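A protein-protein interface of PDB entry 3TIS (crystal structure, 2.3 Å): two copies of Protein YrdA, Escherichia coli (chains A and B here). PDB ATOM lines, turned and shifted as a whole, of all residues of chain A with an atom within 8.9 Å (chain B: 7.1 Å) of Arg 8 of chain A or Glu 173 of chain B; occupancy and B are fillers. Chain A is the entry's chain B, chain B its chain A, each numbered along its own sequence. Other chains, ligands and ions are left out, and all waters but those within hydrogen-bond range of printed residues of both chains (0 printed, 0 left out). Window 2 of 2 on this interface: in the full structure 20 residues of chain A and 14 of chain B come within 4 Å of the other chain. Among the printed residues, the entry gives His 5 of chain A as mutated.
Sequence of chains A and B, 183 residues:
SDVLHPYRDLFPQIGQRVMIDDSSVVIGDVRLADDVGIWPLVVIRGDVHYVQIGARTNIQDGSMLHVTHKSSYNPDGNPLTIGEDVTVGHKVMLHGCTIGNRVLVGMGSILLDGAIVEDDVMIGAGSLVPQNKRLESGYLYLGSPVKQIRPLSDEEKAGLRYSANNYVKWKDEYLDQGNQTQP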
ATOM      1  N   HIS A   5     -39.488 -32.448 -23.826  1.00  0.00           N
ATOM      2  CA  HIS A   5     -38.500 -31.900 -22.907  1.00  0.00           C
ATOM      3  C   HIS A   5     -38.099 -30.474 -23.278  1.00  0.00           C
ATOM      4  O   HIS A   5     -38.055 -30.109 -24.455  1.00  0.00           O
ATOM      5  CB  HIS A   5     -37.254 -32.785 -22.885  1.00  0.00           C
ATOM      6  CG  HIS A   5     -37.550 -34.232 -22.642  1.00  0.00           C
ATOM      7  ND1 HIS A   5     -38.138 -35.041 -23.591  1.00  0.00           N
ATOM      8  CD2 HIS A   5     -37.371 -35.006 -21.546  1.00  0.00           C
ATOM      9  CE1 HIS A   5     -38.310 -36.250 -23.090  1.00  0.00           C
ATOM     10  NE2 HIS A   5     -37.853 -36.255 -21.849  1.00  0.00           N
ATOM     11  N   PRO A   6     -37.800 -29.647 -22.269  1.00  0.00           N
ATOM     12  CA  PRO A   6     -37.408 -28.267 -22.548  1.00  0.00           C
ATOM     13  C   PRO A   6     -35.903 -28.108 -22.729  1.00  0.00           C
ATOM     14  O   PRO A   6     -35.121 -29.023 -22.470  1.00  0.00           O
ATOM     15  CB  PRO A   6     -37.903 -27.525 -21.316  1.00  0.00           C
ATOM     16  CG  PRO A   6     -37.580 -28.503 -20.226  1.00  0.00           C
ATOM     17  CD  PRO A   6     -38.048 -29.835 -20.824  1.00  0.00           C
ATOM     18  N   TYR A   7     -35.525 -26.928 -23.197  1.00  0.00           N
ATOM     19  CA  TYR A   7     -34.135 -26.551 -23.392  1.00  0.00           C
ATOM     20  C   TYR A   7     -34.162 -25.039 -23.209  1.00  0.00           C
ATOM     21  O   TYR A   7     -34.762 -24.325 -24.016  1.00  0.00           O
ATOM     22  CB  TYR A   7     -33.648 -26.894 -24.791  1.00  0.00           C
ATOM     23  CG  TYR A   7     -32.225 -26.456 -24.996  1.00  0.00           C
ATOM     24  CD1 TYR A   7     -31.176 -27.100 -24.337  1.00  0.00           C
ATOM     25  CD2 TYR A   7     -31.926 -25.358 -25.797  1.00  0.00           C
ATOM     26  CE1 TYR A   7     -29.866 -26.655 -24.470  1.00  0.00           C
ATOM     27  CE2 TYR A   7     -30.620 -24.905 -25.935  1.00  0.00           C
ATOM     28  CZ  TYR A   7     -29.597 -25.555 -25.269  1.00  0.00           C
ATOM     29  OH  TYR A   7     -28.310 -25.091 -25.404  1.00  0.00           O
ATOM     30  N   ARG A   8     -33.517 -24.553 -22.153  1.00  0.00           N
ATOM     31  CA  ARG A   8     -33.549 -23.128 -21.854  1.00  0.00           C
ATOM     32  C   ARG A   8     -35.010 -22.849 -21.539  1.00  0.00           C
ATOM     33  O   ARG A   8     -35.623 -23.555 -20.739  1.00  0.00           O
ATOM     34  CB  ARG A   8     -33.109 -22.293 -23.060  1.00  0.00           C
ATOM     35  CG  ARG A   8     -31.661 -21.849 -23.018  1.00  0.00           C
ATOM     36  CD  ARG A   8     -30.708 -23.025 -22.948  1.00  0.00           C
ATOM     37  NE  ARG A   8     -29.320 -22.578 -22.955  1.00  0.00           N
ATOM     38  CZ  ARG A   8     -28.780 -21.833 -23.915  1.00  0.00           C
ATOM     39  NH1 ARG A   8     -29.515 -21.450 -24.951  1.00  0.00           N
ATOM     40  NH2 ARG A   8     -27.509 -21.465 -23.843  1.00  0.00           N
ATOM     41  N   ASP A   9     -35.580 -21.844 -22.186  1.00  0.00           N
ATOM     42  CA  ASP A   9     -36.977 -21.510 -21.955  1.00  0.00           C
ATOM     43  C   ASP A   9     -37.839 -22.101 -23.071  1.00  0.00           C
ATOM     44  O   ASP A   9     -39.061 -22.039 -23.028  1.00  0.00           O
ATOM     45  CB  ASP A   9     -37.141 -19.987 -21.903  1.00  0.00           C
ATOM     46  CG  ASP A   9     -36.221 -19.335 -20.874  1.00  0.00           C
ATOM     47  OD1 ASP A   9     -34.991 -19.535 -20.965  1.00  0.00           O
ATOM     48  OD2 ASP A   9     -36.724 -18.622 -19.976  1.00  0.00           O
ATOM     49  N   LEU A  10     -37.177 -22.696 -24.057  1.00  0.00           N
ATOM     50  CA  LEU A  10     -37.833 -23.292 -25.216  1.00  0.00           C
ATOM     51  C   LEU A  10     -38.520 -24.632 -24.932  1.00  0.00           C
ATOM     52  O   LEU A  10     -37.963 -25.498 -24.261  1.00  0.00           O
ATOM     53  CB  LEU A  10     -36.796 -23.460 -26.324  1.00  0.00           C
ATOM     54  CG  LEU A  10     -35.976 -22.198 -26.607  1.00  0.00           C
ATOM     55  CD1 LEU A  10     -34.867 -22.507 -27.603  1.00  0.00           C
ATOM     56  CD2 LEU A  10     -36.893 -21.109 -27.133  1.00  0.00           C
ATOM     57  N   PHE A  11     -39.728 -24.798 -25.466  1.00  0.00           N
ATOM     58  CA  PHE A  11     -40.511 -26.016 -25.268  1.00  0.00           C
ATOM     59  C   PHE A  11     -41.260 -26.344 -26.558  1.00  0.00           C
ATOM     60  O   PHE A  11     -41.746 -25.451 -27.241  1.00  0.00           O
ATOM     61  CB  PHE A  11     -41.515 -25.804 -24.132  1.00  0.00           C
ATOM     62  CG  PHE A  11     -42.168 -27.066 -23.649  1.00  0.00           C
ATOM     63  CD1 PHE A  11     -41.443 -28.001 -22.914  1.00  0.00           C
ATOM     64  CD2 PHE A  11     -43.510 -27.318 -23.922  1.00  0.00           C
ATOM     65  CE1 PHE A  11     -42.045 -29.169 -22.455  1.00  0.00           C
ATOM     66  CE2 PHE A  11     -44.125 -28.486 -23.469  1.00  0.00           C
ATOM     67  CZ  PHE A  11     -43.392 -29.412 -22.732  1.00  0.00           C
ATOM     68  N   ILE A  27     -37.049 -32.486 -27.923  1.00  0.00           N
ATOM     69  CA  ILE A  27     -36.489 -31.435 -27.075  1.00  0.00           C
ATOM     70  C   ILE A  27     -36.419 -30.029 -27.662  1.00  0.00           C
ATOM     71  O   ILE A  27     -36.150 -29.848 -28.851  1.00  0.00           O
ATOM     72  CB  ILE A  27     -35.048 -31.816 -26.660  1.00  0.00           C
ATOM     73  CG1 ILE A  27     -35.055 -33.157 -25.930  1.00  0.00           C
ATOM     74  CG2 ILE A  27     -34.431 -30.721 -25.796  1.00  0.00           C
ATOM     75  CD1 ILE A  27     -33.679 -33.776 -25.796  1.00  0.00           C
ATOM     76  N   GLY A  28     -36.651 -29.041 -26.800  1.00  0.00           N
ATOM     77  CA  GLY A  28     -36.560 -27.646 -27.194  1.00  0.00           C
ATOM     78  C   GLY A  28     -37.537 -27.050 -28.190  1.00  0.00           C
ATOM     79  O   GLY A  28     -38.715 -27.415 -28.246  1.00  0.00           O
ATOM     80  N   ASP A  29     -37.015 -26.113 -28.978  1.00  0.00           N
ATOM     81  CA  ASP A  29     -37.778 -25.378 -29.980  1.00  0.00           C
ATOM     82  C   ASP A  29     -38.168 -26.242 -31.171  1.00  0.00           C
ATOM     83  O   ASP A  29     -37.594 -26.110 -32.258  1.00  0.00           O
ATOM     84  CB  ASP A  29     -36.955 -24.183 -30.466  1.00  0.00           C
ATOM     85  CG  ASP A  29     -37.809 -23.089 -31.077  1.00  0.00           C
ATOM     86  OD1 ASP A  29     -38.976 -23.362 -31.446  1.00  0.00           O
ATOM     87  OD2 ASP A  29     -37.305 -21.954 -31.197  1.00  0.00           O
ATOM     88  N   ARG A  45     -34.061 -32.961 -31.685  1.00  0.00           N
ATOM     89  CA  ARG A  45     -33.457 -32.031 -30.753  1.00  0.00           C
ATOM     90  C   ARG A  45     -33.276 -30.647 -31.342  1.00  0.00           C
ATOM     91  O   ARG A  45     -32.321 -30.390 -32.068  1.00  0.00           O
ATOM     92  CB  ARG A  45     -32.111 -32.595 -30.286  1.00  0.00           C
ATOM     93  CG  ARG A  45     -31.381 -31.735 -29.285  1.00  0.00           C
ATOM     94  CD  ARG A  45     -30.520 -32.593 -28.370  1.00  0.00           C
ATOM     95  NE  ARG A  45     -29.473 -33.329 -29.075  1.00  0.00           N
ATOM     96  CZ  ARG A  45     -28.244 -32.869 -29.302  1.00  0.00           C
ATOM     97  NH1 ARG A  45     -27.892 -31.663 -28.884  1.00  0.00           N
ATOM     98  NH2 ARG A  45     -27.353 -33.628 -29.925  1.00  0.00           N
ATOM     99  N   GLY A  46     -34.208 -29.754 -31.032  1.00  0.00           N
ATOM    100  CA  GLY A  46     -34.118 -28.395 -31.533  1.00  0.00           C
ATOM    101  C   GLY A  46     -33.626 -27.495 -30.417  1.00  0.00           C
ATOM    102  O   GLY A  46     -34.314 -26.553 -30.023  1.00  0.00           O
ATOM    103  N   ASP A  47     -32.427 -27.781 -29.915  1.00  0.00           N
ATOM    104  CA  ASP A  47     -31.856 -27.015 -28.814  1.00  0.00           C
ATOM    105  C   ASP A  47     -31.025 -25.798 -29.208  1.00  0.00           C
ATOM    106  O   ASP A  47     -31.364 -24.678 -28.833  1.00  0.00           O
ATOM    107  CB  ASP A  47     -31.043 -27.946 -27.897  1.00  0.00           C
ATOM    108  CG  ASP A  47     -30.030 -28.796 -28.654  1.00  0.00           C
ATOM    109  OD1 ASP A  47     -29.487 -29.739 -28.051  1.00  0.00           O
ATOM    110  OD2 ASP A  47     -29.760 -28.528 -29.837  1.00  0.00           O
ATOM    111  N   VAL A  48     -29.945 -26.001 -29.954  1.00  0.00           N
ATOM    112  CA  VAL A  48     -29.102 -24.880 -30.362  1.00  0.00           C
ATOM    113  C   VAL A  48     -29.718 -24.100 -31.525  1.00  0.00           C
ATOM    114  O   VAL A  48     -29.182 -23.084 -31.964  1.00  0.00           O
ATOM    115  CB  VAL A  48     -27.671 -25.356 -30.735  1.00  0.00           C
ATOM    116  CG1 VAL A  48     -26.980 -25.913 -29.498  1.00  0.00           C
ATOM    117  CG2 VAL A  48     -27.729 -26.409 -31.825  1.00  0.00           C
ATOM    118  N   HIS A  49     -30.850 -24.582 -32.016  1.00  0.00           N
ATOM    119  CA  HIS A  49     -31.567 -23.918 -33.100  1.00  0.00           C
ATOM    120  C   HIS A  49     -32.937 -24.576 -33.200  1.00  0.00           C
ATOM    121  O   HIS A  49     -33.168 -25.618 -32.595  1.00  0.00           O
ATOM    122  CB  HIS A  49     -30.809 -24.044 -34.423  1.00  0.00           C
ATOM    123  CG  HIS A  49     -30.764 -22.771 -35.206  1.00  0.00           C
ATOM    124  ND1 HIS A  49     -31.899 -22.063 -35.543  1.00  0.00           N
ATOM    125  CD2 HIS A  49     -29.720 -22.056 -35.690  1.00  0.00           C
ATOM    126  CE1 HIS A  49     -31.556 -20.967 -36.195  1.00  0.00           C
ATOM    127  NE2 HIS A  49     -30.240 -20.938 -36.298  1.00  0.00           N
ATOM    128  N   MET B  19     -23.323 -36.933 -18.047  1.00  0.00           N
ATOM    129  CA  MET B  19     -24.735 -36.955 -18.398  1.00  0.00           C
ATOM    130  C   MET B  19     -25.101 -38.176 -19.221  1.00  0.00           C
ATOM    131  O   MET B  19     -24.382 -38.557 -20.145  1.00  0.00           O
ATOM    132  CB  MET B  19     -25.138 -35.716 -19.200  1.00  0.00           C
ATOM    133  CG  MET B  19     -26.571 -35.807 -19.715  1.00  0.00           C
ATOM    134  SD  MET B  19     -26.973 -34.671 -21.064  1.00  0.00           S
ATOM    135  CE  MET B  19     -26.363 -35.624 -22.482  1.00  0.00           C
ATOM    136  N   ASN B 166     -17.764 -27.400 -26.961  1.00  0.00           N
ATOM    137  CA  ASN B 166     -19.168 -27.028 -27.087  1.00  0.00           C
ATOM    138  C   ASN B 166     -20.082 -28.104 -26.507  1.00  0.00           C
ATOM    139  O   ASN B 166     -20.989 -27.804 -25.738  1.00  0.00           O
ATOM    140  CB  ASN B 166     -19.548 -26.786 -28.553  1.00  0.00           C
ATOM    141  CG  ASN B 166     -18.979 -25.489 -29.099  1.00  0.00           C
ATOM    142  OD1 ASN B 166     -18.895 -24.485 -28.388  1.00  0.00           O
ATOM    143  ND2 ASN B 166     -18.599 -25.498 -30.373  1.00  0.00           N
ATOM    144  N   TYR B 167     -19.841 -29.362 -26.855  1.00  0.00           N
ATOM    145  CA  TYR B 167     -20.699 -30.414 -26.342  1.00  0.00           C
ATOM    146  C   TYR B 167     -20.601 -30.583 -24.832  1.00  0.00           C
ATOM    147  O   TYR B 167     -21.560 -31.025 -24.194  1.00  0.00           O
ATOM    148  CB  TYR B 167     -20.445 -31.740 -27.073  1.00  0.00           C
ATOM    149  CG  TYR B 167     -21.528 -32.030 -28.096  1.00  0.00           C
ATOM    150  CD1 TYR B 167     -21.395 -31.622 -29.422  1.00  0.00           C
ATOM    151  CD2 TYR B 167     -22.730 -32.637 -27.712  1.00  0.00           C
ATOM    152  CE1 TYR B 167     -22.434 -31.805 -30.342  1.00  0.00           C
ATOM    153  CE2 TYR B 167     -23.775 -32.823 -28.619  1.00  0.00           C
ATOM    154  CZ  TYR B 167     -23.623 -32.404 -29.932  1.00  0.00           C
ATOM    155  OH  TYR B 167     -24.663 -32.565 -30.825  1.00  0.00           O
ATOM    156  N   VAL B 168     -19.455 -30.232 -24.257  1.00  0.00           N
ATOM    157  CA  VAL B 168     -19.304 -30.311 -22.811  1.00  0.00           C
ATOM    158  C   VAL B 168     -20.250 -29.263 -22.191  1.00  0.00           C
ATOM    159  O   VAL B 168     -20.940 -29.540 -21.208  1.00  0.00           O
ATOM    160  CB  VAL B 168     -17.841 -30.035 -22.379  1.00  0.00           C
ATOM    161  CG1 VAL B 168     -17.774 -29.760 -20.879  1.00  0.00           C
ATOM    162  CG2 VAL B 168     -16.972 -31.244 -22.711  1.00  0.00           C
ATOM    163  N   LYS B 169     -20.300 -28.071 -22.783  1.00  0.00           N
ATOM    164  CA  LYS B 169     -21.187 -27.023 -22.277  1.00  0.00           C
ATOM    165  C   LYS B 169     -22.660 -27.395 -22.422  1.00  0.00           C
ATOM    166  O   LYS B 169     -23.435 -27.275 -21.467  1.00  0.00           O
ATOM    167  CB  LYS B 169     -20.949 -25.693 -23.003  1.00  0.00           C
ATOM    168  CG  LYS B 169     -19.721 -24.932 -22.543  1.00  0.00           C
ATOM    169  CD  LYS B 169     -19.785 -23.473 -22.974  1.00  0.00           C
ATOM    170  CE  LYS B 169     -18.595 -22.697 -22.437  1.00  0.00           C
ATOM    171  NZ  LYS B 169     -18.674 -21.243 -22.766  1.00  0.00           N
ATOM    172  N   TRP B 170     -23.046 -27.840 -23.617  1.00  0.00           N
ATOM    173  CA  TRP B 170     -24.432 -28.217 -23.878  1.00  0.00           C
ATOM    174  C   TRP B 170     -24.872 -29.318 -22.928  1.00  0.00           C
ATOM    175  O   TRP B 170     -26.001 -29.315 -22.442  1.00  0.00           O
ATOM    176  CB  TRP B 170     -24.602 -28.647 -25.340  1.00  0.00           C
ATOM    177  CG  TRP B 170     -24.309 -27.523 -26.294  1.00  0.00           C
ATOM    178  CD1 TRP B 170     -24.552 -26.190 -26.083  1.00  0.00           C
ATOM    179  CD2 TRP B 170     -23.747 -27.623 -27.611  1.00  0.00           C
ATOM    180  NE1 TRP B 170     -24.176 -25.459 -27.185  1.00  0.00           N
ATOM    181  CE2 TRP B 170     -23.678 -26.310 -28.137  1.00  0.00           C
ATOM    182  CE3 TRP B 170     -23.295 -28.691 -28.398  1.00  0.00           C
ATOM    183  CZ2 TRP B 170     -23.176 -26.036 -29.420  1.00  0.00           C
ATOM    184  CZ3 TRP B 170     -22.796 -28.419 -29.676  1.00  0.00           C
ATOM    185  CH2 TRP B 170     -22.740 -27.099 -30.172  1.00  0.00           C
ATOM    186  N   LYS B 171     -23.971 -30.255 -22.663  1.00  0.00           N
ATOM    187  CA  LYS B 171     -24.248 -31.343 -21.737  1.00  0.00           C
ATOM    188  C   LYS B 171     -24.596 -30.773 -20.359  1.00  0.00           C
ATOM    189  O   LYS B 171     -25.579 -31.176 -19.737  1.00  0.00           O
ATOM    190  CB  LYS B 171     -23.018 -32.237 -21.607  1.00  0.00           C
ATOM    191  CG  LYS B 171     -23.065 -33.157 -20.411  1.00  0.00           C
ATOM    192  CD  LYS B 171     -21.666 -33.430 -19.854  1.00  0.00           C
ATOM    193  CE  LYS B 171     -21.077 -32.191 -19.199  1.00  0.00           C
ATOM    194  NZ  LYS B 171     -19.813 -32.486 -18.467  1.00  0.00           N
ATOM    195  N   ASP B 172     -23.781 -29.834 -19.883  1.00  0.00           N
ATOM    196  CA  ASP B 172     -24.008 -29.230 -18.576  1.00  0.00           C
ATOM    197  C   ASP B 172     -25.307 -28.432 -18.502  1.00  0.00           C
ATOM    198  O   ASP B 172     -25.885 -28.275 -17.426  1.00  0.00           O
ATOM    199  CB  ASP B 172     -22.821 -28.346 -18.171  1.00  0.00           C
ATOM    200  CG  ASP B 172     -21.606 -29.157 -17.749  1.00  0.00           C
ATOM    201  OD1 ASP B 172     -21.782 -30.129 -16.988  1.00  0.00           O
ATOM    202  OD2 ASP B 172     -20.473 -28.822 -18.164  1.00  0.00           O
ATOM    203  N   GLU B 173     -25.773 -27.926 -19.636  1.00  0.00           N
ATOM    204  CA  GLU B 173     -27.018 -27.179 -19.627  1.00  0.00           C
ATOM    205  C   GLU B 173     -28.148 -28.143 -19.334  1.00  0.00           C
ATOM    206  O   GLU B 173     -29.135 -27.785 -18.693  1.00  0.00           O
ATOM    207  CB  GLU B 173     -27.247 -26.485 -20.964  1.00  0.00           C
ATOM    208  CG  GLU B 173     -26.311 -25.321 -21.181  1.00  0.00           C
ATOM    209  CD  GLU B 173     -26.725 -24.456 -22.343  1.00  0.00           C
ATOM    210  OE1 GLU B 173     -26.630 -24.917 -23.494  1.00  0.00           O
ATOM    211  OE2 GLU B 173     -27.155 -23.312 -22.101  1.00  0.00           O
ATOM    212  N   TYR B 174     -28.003 -29.376 -19.802  1.00  0.00           N
ATOM    213  CA  TYR B 174     -29.027 -30.377 -19.545  1.00  0.00           C
ATOM    214  C   TYR B 174     -28.898 -30.824 -18.096  1.00  0.00           C
ATOM    215  O   TYR B 174     -29.899 -31.073 -17.422  1.00  0.00           O
ATOM    216  CB  TYR B 174     -28.876 -31.565 -20.503  1.00  0.00           C
ATOM    217  CG  TYR B 174     -29.520 -31.321 -21.848  1.00  0.00           C
ATOM    218  CD1 TYR B 174     -30.886 -31.522 -22.038  1.00  0.00           C
ATOM    219  CD2 TYR B 174     -28.775 -30.814 -22.909  1.00  0.00           C
ATOM    220  CE1 TYR B 174     -31.496 -31.217 -23.255  1.00  0.00           C
ATOM    221  CE2 TYR B 174     -29.370 -30.504 -24.127  1.00  0.00           C
ATOM    222  CZ  TYR B 174     -30.727 -30.704 -24.295  1.00  0.00           C
ATOM    223  OH  TYR B 174     -31.305 -30.375 -25.502  1.00  0.00           O
ATOM    224  N   LEU B 175     -27.664 -30.913 -17.611  1.00  0.00           N
ATOM    225  CA  LEU B 175     -27.441 -31.314 -16.228  1.00  0.00           C
ATOM    226  C   LEU B 175     -28.021 -30.239 -15.319  1.00  0.00           C
ATOM    227  O   LEU B 175     -28.506 -30.528 -14.226  1.00  0.00           O
ATOM    228  CB  LEU B 175     -25.946 -31.489 -15.940  1.00  0.00           C
ATOM    229  CG  LEU B 175     -25.234 -32.608 -16.700  1.00  0.00           C
ATOM    230  CD1 LEU B 175     -23.775 -32.694 -16.263  1.00  0.00           C
ATOM    231  CD2 LEU B 175     -25.947 -33.915 -16.438  1.00  0.00           C
ATOM    232  N   ASP B 176     -27.983 -28.995 -15.782  1.00  0.00           N
ATOM    233  CA  ASP B 176     -28.511 -27.900 -14.990  1.00  0.00           C
ATOM    234  C   ASP B 176     -30.034 -27.978 -14.887  1.00  0.00           C
ATOM    235  O   ASP B 176     -30.589 -27.940 -13.788  1.00  0.00           O
ATOM    236  CB  ASP B 176     -28.099 -26.559 -15.591  1.00  0.00           C
ATOM    237  CG  ASP B 176     -28.532 -25.390 -14.737  1.00  0.00           C
ATOM    238  OD1 ASP B 176     -28.107 -25.334 -13.559  1.00  0.00           O
ATOM    239  OD2 ASP B 176     -29.299 -24.536 -15.236  1.00  0.00           O
ATOM    240  N   GLN B 177     -30.704 -28.092 -16.031  1.00  0.00           N
ATOM    241  CA  GLN B 177     -32.167 -28.170 -16.057  1.00  0.00           C
ATOM    242  C   GLN B 177     -32.686 -29.303 -15.179  1.00  0.00           C
ATOM    243  O   GLN B 177     -33.761 -29.197 -14.584  1.00  0.00           O
ATOM    244  CB  GLN B 177     -32.667 -28.355 -17.496  1.00  0.00           C
ATOM    245  CG  GLN B 177     -32.320 -27.189 -18.415  1.00  0.00           C
ATOM    246  CD  GLN B 177     -32.765 -27.404 -19.852  1.00  0.00           C
ATOM    247  OE1 GLN B 177     -32.497 -26.575 -20.724  1.00  0.00           O
ATOM    248  NE2 GLN B 177     -33.445 -28.517 -20.105  1.00  0.00           N
ATOM    249  N   GLY B 178     -31.915 -30.384 -15.095  1.00  0.00           N
ATOM    250  CA  GLY B 178     -32.301 -31.530 -14.283  1.00  0.00           C
ATOM    251  C   GLY B 178     -32.164 -31.188 -12.806  1.00  0.00           C
ATOM    252  O   GLY B 178     -33.158 -31.108 -12.083  1.00  0.00           O
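OH of Tyr 167 of chain B sits at hydrogen-bond distance from NH2 of Arg 45 of chain A.
OH of Tyr 7 of chain A is in hydrogen-bond range of OE1 of Glu 173 of chain B (2.5 Å).
OE2 of Glu 173 of chain B is in salt-bridge range of NE of Arg 8 of chain A.
The side-chain carboxylate of Asp 47 of chain A lies within hydrogen-bond range of the side-chain hydroxyl of Tyr 174 of chain B.
NE2 of Gln 177 of chain B is in hydrogen-bond range of O of Pro 6 of chain A (2.9 Å).
N of Arg 8 of chain A lies within hydrogen-bond range of OE1 of Gln 177 of chain B (2.7 Å).
The backbone carbonyl oxygen (O) of Ile 27 of chain A lies within hydrogen-bond range of the backbone NH (N) of Gly 46 of chain A (2.9 Å).
The guanidinium group (NH1) of Arg 45 of chain A is in salt-bridge range of the side-chain carboxylate (OD1) of Asp 47 of chain A, 2.6 Å away.
Among the printed residues, merely in contact across the chains: Tyr 7 of chain A with Gln 177 of chain B, Ile 27 of chain A with Tyr 174 of chain B, Tyr 7 of chain A with Tyr 174 of chain B, Val 48 of chain A with Trp 170 of chain B, Arg 45 of chain A with Tyr 174 of chain B and Tyr 7 of chain A with Trp 170 of chain B.
Arg 8 of chain A touches just these residues of chain B: Glu 173 and Gln 177.
Of chain A, only Tyr 7 and Arg 8 come within 4 Å of Glu 173 of chain B.
Printed residues of chain B within 4 Å of Pro 6 of chain A: Gln 177.
Printed residues of chain A within 4 Å of Tyr 167 of chain B: Arg 45 (3.0 Å).
Of the printed residues of chain B, Val 48 of chain A touches Trp 170.
Of the printed residues of chain B, Ile 27 of chain A touches Tyr 174 (3.2 Å).
Of the printed residues of chain B, Tyr 7 of chain A touches Trp 170, Glu 173, Tyr 174 and Gln 177.
His 49 of chain A touches none of the printed residues of chain B.
The nearest residue of chain B that does not touch Arg 8 of chain A is Trp 170 of chain B (6.0 Å).
Of the 15 printed residues of chain A, 7 touch a printed residue of chain B.
Among the printed residues, Asp or Glu carboxylates within 4 Å of a Lys or Arg side-chain nitrogen of the other chain: Arg 8 of chain A with Glu 173 of chain B (2.4 Å).
No position is printed for both chains.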
